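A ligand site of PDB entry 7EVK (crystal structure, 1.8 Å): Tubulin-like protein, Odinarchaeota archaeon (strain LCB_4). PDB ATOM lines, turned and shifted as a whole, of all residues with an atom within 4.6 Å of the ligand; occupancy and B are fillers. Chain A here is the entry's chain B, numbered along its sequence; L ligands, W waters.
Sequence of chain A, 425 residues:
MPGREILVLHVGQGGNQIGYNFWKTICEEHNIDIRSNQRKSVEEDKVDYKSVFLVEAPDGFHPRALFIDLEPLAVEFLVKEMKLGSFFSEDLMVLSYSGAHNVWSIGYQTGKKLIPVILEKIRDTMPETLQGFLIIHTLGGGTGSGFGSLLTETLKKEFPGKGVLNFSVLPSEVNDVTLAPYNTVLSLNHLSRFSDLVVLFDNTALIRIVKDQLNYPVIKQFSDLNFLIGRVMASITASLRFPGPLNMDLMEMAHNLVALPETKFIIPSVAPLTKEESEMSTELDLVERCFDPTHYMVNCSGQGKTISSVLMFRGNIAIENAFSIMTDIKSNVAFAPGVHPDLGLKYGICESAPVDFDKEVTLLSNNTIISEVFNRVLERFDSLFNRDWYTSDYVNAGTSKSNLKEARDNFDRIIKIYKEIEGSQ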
ATOM      1  N   VAL A  11     -24.509   0.712 -13.189  1.00  0.00           N
ATOM      2  CA  VAL A  11     -23.866   1.417 -12.080  1.00  0.00           C
ATOM      3  C   VAL A  11     -24.209   2.909 -12.141  1.00  0.00           C
ATOM      4  O   VAL A  11     -23.905   3.566 -13.140  1.00  0.00           O
ATOM      5  CB  VAL A  11     -22.340   1.229 -12.084  1.00  0.00           C
ATOM      6  CG1 VAL A  11     -21.747   1.762 -10.784  1.00  0.00           C
ATOM      7  CG2 VAL A  11     -21.978  -0.257 -12.253  1.00  0.00           C
ATOM      8  N   GLY A  12     -24.814   3.426 -11.050  1.00  0.00           N
ATOM      9  CA  GLY A  12     -25.151   4.843 -10.933  1.00  0.00           C
ATOM     10  C   GLY A  12     -26.434   5.203 -11.683  1.00  0.00           C
ATOM     11  O   GLY A  12     -27.111   4.348 -12.268  1.00  0.00           O
ATOM     12  N   GLN A  13     -26.777   6.501 -11.652  1.00  0.00           N
ATOM     13  CA  GLN A  13     -28.062   6.918 -12.220  1.00  0.00           C
ATOM     14  C   GLN A  13     -28.125   6.584 -13.698  1.00  0.00           C
ATOM     15  O   GLN A  13     -29.045   5.902 -14.160  1.00  0.00           O
ATOM     16  CB  GLN A  13     -28.328   8.420 -12.004  1.00  0.00           C
ATOM     17  CG  GLN A  13     -29.647   8.903 -12.704  1.00  0.00           C
ATOM     18  CD  GLN A  13     -30.365  10.041 -11.976  1.00  0.00           C
ATOM     19  OE1 GLN A  13     -29.723  10.825 -11.278  1.00  0.00           O
ATOM     20  NE2 GLN A  13     -31.695  10.126 -12.127  1.00  0.00           N
ATOM     21  N   GLY A  14     -27.133   7.067 -14.466  1.00  0.00           N
ATOM     22  CA  GLY A  14     -27.176   6.841 -15.905  1.00  0.00           C
ATOM     23  C   GLY A  14     -27.124   5.369 -16.258  1.00  0.00           C
ATOM     24  O   GLY A  14     -27.881   4.895 -17.110  1.00  0.00           O
ATOM     25  N   GLN A  17     -30.556   3.804 -15.579  1.00  0.00           N
ATOM     26  CA  GLN A  17     -31.587   4.295 -16.497  1.00  0.00           C
ATOM     27  C   GLN A  17     -31.392   3.694 -17.897  1.00  0.00           C
ATOM     28  O   GLN A  17     -32.370   3.308 -18.554  1.00  0.00           O
ATOM     29  CB  GLN A  17     -31.594   5.820 -16.480  1.00  0.00           C
ATOM     30  CG  GLN A  17     -32.165   6.309 -15.161  1.00  0.00           C
ATOM     31  CD  GLN A  17     -32.172   7.816 -14.924  1.00  0.00           C
ATOM     32  OE1 GLN A  17     -32.802   8.252 -13.967  1.00  0.00           O
ATOM     33  NE2 GLN A  17     -31.441   8.606 -15.741  1.00  0.00           N
ATOM     34  N   ILE A  18     -30.138   3.545 -18.331  1.00  0.00           N
ATOM     35  CA  ILE A  18     -29.848   2.893 -19.610  1.00  0.00           C
ATOM     36  C   ILE A  18     -30.311   1.445 -19.566  1.00  0.00           C
ATOM     37  O   ILE A  18     -30.836   0.901 -20.554  1.00  0.00           O
ATOM     38  CB  ILE A  18     -28.353   3.014 -19.939  1.00  0.00           C
ATOM     39  CG1 ILE A  18     -27.984   4.459 -20.226  1.00  0.00           C
ATOM     40  CG2 ILE A  18     -27.975   2.092 -21.132  1.00  0.00           C
ATOM     41  CD1 ILE A  18     -26.463   4.707 -20.120  1.00  0.00           C
ATOM     42  N   ASP A  69     -26.149   1.089  -7.114  1.00  0.00           N
ATOM     43  CA  ASP A  69     -26.005   2.542  -6.965  1.00  0.00           C
ATOM     44  C   ASP A  69     -25.691   2.831  -5.504  1.00  0.00           C
ATOM     45  O   ASP A  69     -26.001   2.038  -4.617  1.00  0.00           O
ATOM     46  CB  ASP A  69     -27.277   3.279  -7.410  1.00  0.00           C
ATOM     47  CG  ASP A  69     -27.021   4.700  -7.894  1.00  0.00           C
ATOM     48  OD1 ASP A  69     -25.984   5.321  -7.524  1.00  0.00           O
ATOM     49  OD2 ASP A  69     -27.864   5.230  -8.652  1.00  0.00           O
ATOM     50  N   GLY A  99     -24.704   8.392  -1.502  1.00  0.00           N
ATOM     51  CA  GLY A  99     -24.328   9.037  -2.756  1.00  0.00           C
ATOM     52  C   GLY A  99     -22.833   9.285  -2.873  1.00  0.00           C
ATOM     53  O   GLY A  99     -22.112   9.364  -1.883  1.00  0.00           O
ATOM     54  N   ALA A 100     -22.332   9.384  -4.119  1.00  0.00           N
ATOM     55  CA  ALA A 100     -20.914   9.715  -4.294  1.00  0.00           C
ATOM     56  C   ALA A 100     -20.677  11.209  -4.512  1.00  0.00           C
ATOM     57  O   ALA A 100     -19.515  11.616  -4.629  1.00  0.00           O
ATOM     58  CB  ALA A 100     -20.298   8.953  -5.478  1.00  0.00           C
ATOM     59  N   HIS A 101     -21.733  12.029  -4.591  1.00  0.00           N
ATOM     60  CA  HIS A 101     -21.592  13.488  -4.665  1.00  0.00           C
ATOM     61  C   HIS A 101     -20.666  13.913  -5.791  1.00  0.00           C
ATOM     62  O   HIS A 101     -19.918  14.894  -5.676  1.00  0.00           O
ATOM     63  CB  HIS A 101     -21.099  14.057  -3.333  1.00  0.00           C
ATOM     64  CG  HIS A 101     -21.812  13.480  -2.148  1.00  0.00           C
ATOM     65  ND1 HIS A 101     -23.185  13.459  -2.042  1.00  0.00           N
ATOM     66  CD2 HIS A 101     -21.342  12.898  -1.014  1.00  0.00           C
ATOM     67  CE1 HIS A 101     -23.534  12.896  -0.902  1.00  0.00           C
ATOM     68  NE2 HIS A 101     -22.433  12.536  -0.261  1.00  0.00           N
ATOM     69  N   ASN A 102     -20.718  13.155  -6.900  1.00  0.00           N
ATOM     70  CA  ASN A 102     -20.020  13.447  -8.156  1.00  0.00           C
ATOM     71  C   ASN A 102     -18.497  13.407  -8.018  1.00  0.00           C
ATOM     72  O   ASN A 102     -17.787  14.049  -8.784  1.00  0.00           O
ATOM     73  CB  ASN A 102     -20.430  14.816  -8.717  1.00  0.00           C
ATOM     74  CG  ASN A 102     -21.764  14.792  -9.441  1.00  0.00           C
ATOM     75  OD1 ASN A 102     -22.465  13.758  -9.557  1.00  0.00           O
ATOM     76  ND2 ASN A 102     -22.134  15.960  -9.919  1.00  0.00           N
ATOM     77  N   THR A 138     -22.067   5.912 -16.559  1.00  0.00           N
ATOM     78  CA  THR A 138     -21.544   7.190 -17.022  1.00  0.00           C
ATOM     79  C   THR A 138     -20.201   7.455 -16.382  1.00  0.00           C
ATOM     80  O   THR A 138     -19.875   6.945 -15.300  1.00  0.00           O
ATOM     81  CB  THR A 138     -22.503   8.337 -16.695  1.00  0.00           C
ATOM     82  OG1 THR A 138     -22.504   8.557 -15.281  1.00  0.00           O
ATOM     83  CG2 THR A 138     -23.931   7.977 -17.168  1.00  0.00           C
ATOM     84  N   GLY A 140     -19.045  10.807 -15.991  1.00  0.00           N
ATOM     85  CA  GLY A 140     -18.879  12.166 -15.499  1.00  0.00           C
ATOM     86  C   GLY A 140     -19.361  12.377 -14.070  1.00  0.00           C
ATOM     87  O   GLY A 140     -18.993  13.384 -13.438  1.00  0.00           O
ATOM     88  N   GLY A 141     -20.208  11.471 -13.579  1.00  0.00           N
ATOM     89  CA  GLY A 141     -20.668  11.491 -12.190  1.00  0.00           C
ATOM     90  C   GLY A 141     -19.645  10.805 -11.304  1.00  0.00           C
ATOM     91  O   GLY A 141     -18.482  10.639 -11.674  1.00  0.00           O
ATOM     92  N   GLY A 142     -20.086  10.412 -10.109  1.00  0.00           N
ATOM     93  CA  GLY A 142     -19.167   9.821  -9.134  1.00  0.00           C
ATOM     94  C   GLY A 142     -19.328   8.319  -8.896  1.00  0.00           C
ATOM     95  O   GLY A 142     -18.364   7.634  -8.569  1.00  0.00           O
ATOM     96  N   THR A 143     -20.546   7.806  -9.033  1.00  0.00           N
ATOM     97  CA  THR A 143     -20.797   6.390  -8.752  1.00  0.00           C
ATOM     98  C   THR A 143     -20.523   5.524  -9.983  1.00  0.00           C
ATOM     99  O   THR A 143     -19.697   4.598  -9.927  1.00  0.00           O
ATOM    100  CB  THR A 143     -22.246   6.186  -8.284  1.00  0.00           C
ATOM    101  OG1 THR A 143     -22.457   6.873  -7.032  1.00  0.00           O
ATOM    102  CG2 THR A 143     -22.537   4.706  -8.084  1.00  0.00           C
ATOM    103  N   GLY A 144     -21.195   5.815 -11.093  1.00  0.00           N
ATOM    104  CA  GLY A 144     -20.861   5.152 -12.344  1.00  0.00           C
ATOM    105  C   GLY A 144     -19.380   5.239 -12.640  1.00  0.00           C
ATOM    106  O   GLY A 144     -18.754   4.240 -13.017  1.00  0.00           O
ATOM    107  N   VAL A 169     -20.536   6.301 -20.867  1.00  0.00           N
ATOM    108  CA  VAL A 169     -21.019   7.589 -21.363  1.00  0.00           C
ATOM    109  C   VAL A 169     -20.046   8.705 -20.999  1.00  0.00           C
ATOM    110  O   VAL A 169     -19.856   9.029 -19.820  1.00  0.00           O
ATOM    111  CB  VAL A 169     -22.420   7.889 -20.826  1.00  0.00           C
ATOM    112  CG1 VAL A 169     -22.936   9.182 -21.494  1.00  0.00           C
ATOM    113  CG2 VAL A 169     -23.347   6.687 -21.124  1.00  0.00           C
ATOM    114  N   ASP A 176     -22.027  18.803 -18.071  1.00  0.00           N
ATOM    115  CA  ASP A 176     -23.073  19.170 -17.133  1.00  0.00           C
ATOM    116  C   ASP A 176     -22.746  18.734 -15.702  1.00  0.00           C
ATOM    117  O   ASP A 176     -23.616  18.696 -14.836  1.00  0.00           O
ATOM    118  CB  ASP A 176     -24.438  18.615 -17.580  1.00  0.00           C
ATOM    119  CG  ASP A 176     -24.490  17.118 -17.603  1.00  0.00           C
ATOM    120  OD1 ASP A 176     -23.452  16.479 -17.870  1.00  0.00           O
ATOM    121  OD2 ASP A 176     -25.597  16.582 -17.338  1.00  0.00           O
ATOM    122  N   VAL A 177     -21.478  18.396 -15.459  1.00  0.00           N
ATOM    123  CA  VAL A 177     -20.899  18.185 -14.133  1.00  0.00           C
ATOM    124  C   VAL A 177     -19.533  18.852 -14.194  1.00  0.00           C
ATOM    125  O   VAL A 177     -18.685  18.433 -14.988  1.00  0.00           O
ATOM    126  CB  VAL A 177     -20.732  16.696 -13.782  1.00  0.00           C
ATOM    127  CG1 VAL A 177     -20.053  16.537 -12.433  1.00  0.00           C
ATOM    128  CG2 VAL A 177     -22.061  15.957 -13.842  1.00  0.00           C
ATOM    129  N   ASN A 203     -23.737  12.403 -24.751  1.00  0.00           N
ATOM    130  CA  ASN A 203     -25.087  12.909 -24.948  1.00  0.00           C
ATOM    131  C   ASN A 203     -25.183  13.959 -26.046  1.00  0.00           C
ATOM    132  O   ASN A 203     -26.252  14.137 -26.627  1.00  0.00           O
ATOM    133  CB  ASN A 203     -25.623  13.473 -23.639  1.00  0.00           C
ATOM    134  CG  ASN A 203     -25.898  12.381 -22.653  1.00  0.00           C
ATOM    135  OD1 ASN A 203     -25.996  11.216 -23.031  1.00  0.00           O
ATOM    136  ND2 ASN A 203     -25.991  12.730 -21.383  1.00  0.00           N
ATOM    137  N   LEU A 206     -25.773  11.816 -28.976  1.00  0.00           N
ATOM    138  CA  LEU A 206     -27.055  11.112 -28.892  1.00  0.00           C
ATOM    139  C   LEU A 206     -28.215  12.070 -29.129  1.00  0.00           C
ATOM    140  O   LEU A 206     -29.180  11.725 -29.843  1.00  0.00           O
ATOM    141  CB  LEU A 206     -27.200  10.430 -27.533  1.00  0.00           C
ATOM    142  CG  LEU A 206     -26.203   9.313 -27.236  1.00  0.00           C
ATOM    143  CD1 LEU A 206     -26.368   8.825 -25.794  1.00  0.00           C
ATOM    144  CD2 LEU A 206     -26.305   8.148 -28.261  1.00  0.00           C
ATOM    145  N   PHE A 222     -34.865  10.565 -20.195  1.00  0.00           N
ATOM    146  CA  PHE A 222     -33.683   9.944 -20.772  1.00  0.00           C
ATOM    147  C   PHE A 222     -34.005   8.673 -21.540  1.00  0.00           C
ATOM    148  O   PHE A 222     -33.158   8.203 -22.323  1.00  0.00           O
ATOM    149  CB  PHE A 222     -32.638   9.604 -19.726  1.00  0.00           C
ATOM    150  CG  PHE A 222     -31.618  10.668 -19.520  1.00  0.00           C
ATOM    151  CD1 PHE A 222     -30.789  11.065 -20.555  1.00  0.00           C
ATOM    152  CD2 PHE A 222     -31.446  11.248 -18.277  1.00  0.00           C
ATOM    153  CE1 PHE A 222     -29.818  12.054 -20.373  1.00  0.00           C
ATOM    154  CE2 PHE A 222     -30.467  12.225 -18.065  1.00  0.00           C
ATOM    155  CZ  PHE A 222     -29.655  12.636 -19.121  1.00  0.00           C
ATOM    156  N   ASN A 226     -31.594   7.034 -24.218  1.00  0.00           N
ATOM    157  CA  ASN A 226     -30.890   5.804 -23.895  1.00  0.00           C
ATOM    158  C   ASN A 226     -31.231   4.652 -24.832  1.00  0.00           C
ATOM    159  O   ASN A 226     -30.470   3.687 -24.907  1.00  0.00           O
ATOM    160  CB  ASN A 226     -31.223   5.399 -22.450  1.00  0.00           C
ATOM    161  CG  ASN A 226     -30.666   6.358 -21.453  1.00  0.00           C
ATOM    162  OD1 ASN A 226     -29.677   7.069 -21.754  1.00  0.00           O
ATOM    163  ND2 ASN A 226     -31.261   6.382 -20.269  1.00  0.00           N
ATOM    164  N   ILE A 229     -28.341   3.586 -26.971  1.00  0.00           N
ATOM    165  CA  ILE A 229     -27.337   2.742 -26.330  1.00  0.00           C
ATOM    166  C   ILE A 229     -27.824   1.305 -26.230  1.00  0.00           C
ATOM    167  O   ILE A 229     -27.066   0.356 -26.510  1.00  0.00           O
ATOM    168  CB  ILE A 229     -26.991   3.316 -24.945  1.00  0.00           C
ATOM    169  CG1 ILE A 229     -26.473   4.746 -25.104  1.00  0.00           C
ATOM    170  CG2 ILE A 229     -25.940   2.480 -24.236  1.00  0.00           C
ATOM    171  CD1 ILE A 229     -26.206   5.461 -23.750  1.00  0.00           C
HETATM  172  P1  LIG L   1     -23.313  10.271  -8.352  1.00  0.00           P
HETATM  173  O1  LIG L   1     -22.249  11.319  -8.251  1.00  0.00           O
HETATM  174  O2  LIG L   1     -24.686  10.896  -8.569  1.00  0.00           O
HETATM  175  O3  LIG L   1     -23.236   9.392  -7.144  1.00  0.00           O
HETATM  176  O4  LIG L   1     -22.902   9.334  -9.610  1.00  0.00           O
HETATM  177  P2  LIG L   1     -23.866   8.769 -10.755  1.00  0.00           P
HETATM  178  O5  LIG L   1     -23.102   7.674 -11.423  1.00  0.00           O
HETATM  179  O6  LIG L   1     -25.214   8.318 -10.253  1.00  0.00           O
HETATM  180  O7  LIG L   1     -23.995  10.067 -11.680  1.00  0.00           O
HETATM  181  P3  LIG L   1     -24.817  10.206 -13.040  1.00  0.00           P
HETATM  182  O8  LIG L   1     -25.070   8.868 -13.648  1.00  0.00           O
HETATM  183  O9  LIG L   1     -26.030  11.075 -12.828  1.00  0.00           O
HETATM  184  O10 LIG L   1     -23.697  10.958 -13.927  1.00  0.00           O
HETATM  185  C1  LIG L   1     -23.801  12.272 -14.415  1.00  0.00           C
HETATM  186  C2  LIG L   1     -23.550  12.210 -15.920  1.00  0.00           C
HETATM  187  O11 LIG L   1     -24.357  11.190 -16.503  1.00  0.00           O
HETATM  188  C3  LIG L   1     -23.970  13.519 -16.511  1.00  0.00           C
HETATM  189  O12 LIG L   1     -23.087  13.858 -17.571  1.00  0.00           O
HETATM  190  C4  LIG L   1     -25.390  13.208 -16.944  1.00  0.00           C
HETATM  191  O13 LIG L   1     -25.887  14.041 -17.952  1.00  0.00           O
HETATM  192  C5  LIG L   1     -25.292  11.764 -17.389  1.00  0.00           C
HETATM  193  N1  LIG L   1     -26.494  10.948 -17.227  1.00  0.00           N
HETATM  194  C6  LIG L   1     -27.189  10.672 -16.066  1.00  0.00           C
HETATM  195  N2  LIG L   1     -28.184   9.799 -16.370  1.00  0.00           N
HETATM  196  C7  LIG L   1     -28.102   9.492 -17.691  1.00  0.00           C
HETATM  197  C8  LIG L   1     -28.837   8.657 -18.518  1.00  0.00           C
HETATM  198  O14 LIG L   1     -29.786   8.021 -18.087  1.00  0.00           O
HETATM  199  N3  LIG L   1     -28.489   8.547 -19.860  1.00  0.00           N
HETATM  200  C9  LIG L   1     -27.436   9.268 -20.365  1.00  0.00           C
HETATM  201  N4  LIG L   1     -27.108   9.179 -21.660  1.00  0.00           N
HETATM  202  N5  LIG L   1     -26.714  10.102 -19.542  1.00  0.00           N
HETATM  203  C10 LIG L   1     -27.040  10.201 -18.226  1.00  0.00           C
HETATM  204  O   HOH W   1     -25.251  13.481 -11.403  1.00  0.00           O
HETATM  205  O   HOH W   2     -28.147   7.932  -8.737  1.00  0.00           O
HETATM  206  O   HOH W   3     -25.507   7.984  -7.320  1.00  0.00           O
HETATM  207  O   HOH W   4     -23.937   5.992 -14.230  1.00  0.00           O
HETATM  208  O   HOH W   5     -21.178  15.928 -19.490  1.00  0.00           O
HETATM  209  O   HOH W   6     -27.225  10.941 -10.397  1.00  0.00           O
HETATM  210  O   HOH W   7     -24.122  15.073 -20.405  1.00  0.00           O
HETATM  211  O   HOH W   8     -20.798  11.399 -18.331  1.00  0.00           O
HETATM  212  O   HOH W   9     -20.780   8.432 -12.964  1.00  0.00           O
HETATM  213  O   HOH W  10     -20.573  13.911 -17.582  1.00  0.00           O
HETATM  214  O   HOH W  11     -22.844  12.165 -19.595  1.00  0.00           O
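Residues that only touch the ligand: Gly 12 (3.5 Å), His 101 (3.8 Å), Gly 141 (3.5 Å) and Phe 222 (3.5 Å).
Hydrophobic or aromatic side chains within 4 Å of the ligand: Ala 100 and Phe 222.
16 residues have an atom within 4 Å of the ligand: Gly 12, Gln 13, Gly 14, Gln 17, Ala 100, His 101, Asn 102, Thr 138, Gly 141, Gly 142, Thr 143, Gly 144, Asp 176, Asn 203, Phe 222 and Asn 226.
The side-chain amide nitrogen (ND2) of Asn 226 lies close to the backbone carbonyl oxygen (O) of Phe 222, 3.3 Å away.
The side-chain amide nitrogen (NE2) of Gln 13 is in hydrogen-bond range of the side-chain amide oxygen (OE1) of Gln 17 (2.9 Å).
OD2 of Asp 69 is in hydrogen-bond range of N of Gln 13.
Water W3 lies within hydrogen-bond range of an oxygen (O3) of the ligand (2.7 Å), the side-chain carboxylate of Asp 69 (2.7 Å) and the side-chain hydroxyl of Thr 143 (3.3 Å).
Water W9 lies within hydrogen-bond range of O5 of the ligand (2.9 Å), OG1 of Thr 138 (2.9 Å), N of Gly 141 (3.2 Å) and N of Gly 144 (3.2 Å).
Water W1 bridges an oxygen (O9) of the ligand (2.9 Å) and the side-chain amide oxygen (OD1) of Asn 102 (3.4 Å).
Water W7 lies within hydrogen-bond range of the side-chain carboxylate of Asp 176, the side-chain amide nitrogen of Asn 203 and an oxygen (O13) of the ligand.
Water W2 lies within hydrogen-bond range of the side-chain carboxylate (OD2) of Asp 69 (2.7 Å) and an oxygen (O6) of the ligand (3.3 Å).
Water W8 lies within hydrogen-bond range of the backbone carbonyl oxygen (O) of Val 169, the backbone NH (N) of Gly 140 and an oxygen (O12) of the ligand.
OD2 of Asp 176 sits at hydrogen-bond distance from O13 of the ligand (2.6 Å).
N of Thr 143 lies within hydrogen-bond range of O4 of the ligand (2.9 Å).
The side-chain hydroxyl (OG1) of Thr 143 is in hydrogen-bond range of an oxygen (O3) of the ligand (2.6 Å).
The side-chain amide oxygen (OD1) of Asn 226 lies within hydrogen-bond range of a nitrogen (N3) of the ligand, at 2.7 Å.
An oxygen (O5) of the ligand is in hydrogen-bond range of the backbone NH (N) of Gly 144.
OD1 of Asn 203 sits at hydrogen-bond distance from N4 of the ligand (2.7 Å).
O1 of the ligand sits at hydrogen-bond distance from N of Asn 102.
OD1 of Asn 102 lies close to O1 of the ligand, at 2.8 Å.
The backbone NH (N) of Gln 13 lies within hydrogen-bond range of an oxygen (O6) of the ligand, 2.8 Å away.
N of Gly 14 lies within hydrogen-bond range of O8 of the ligand, at 2.9 Å.
The side-chain amide nitrogen (NE2) of Gln 17 is in hydrogen-bond range of an oxygen (O14) of the ligand, 2.9 Å away.
The backbone NH of Gly 142 is in hydrogen-bond range of an oxygen (O1) of the ligand, 3.0 Å away.
The side-chain hydroxyl (OG1) of Thr 138 is in hydrogen-bond range of an oxygen (O10) of the ligand, at 3.0 Å.
The backbone NH of Ala 100 sits at hydrogen-bond distance from an oxygen (O3) of the ligand (3.2 Å).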
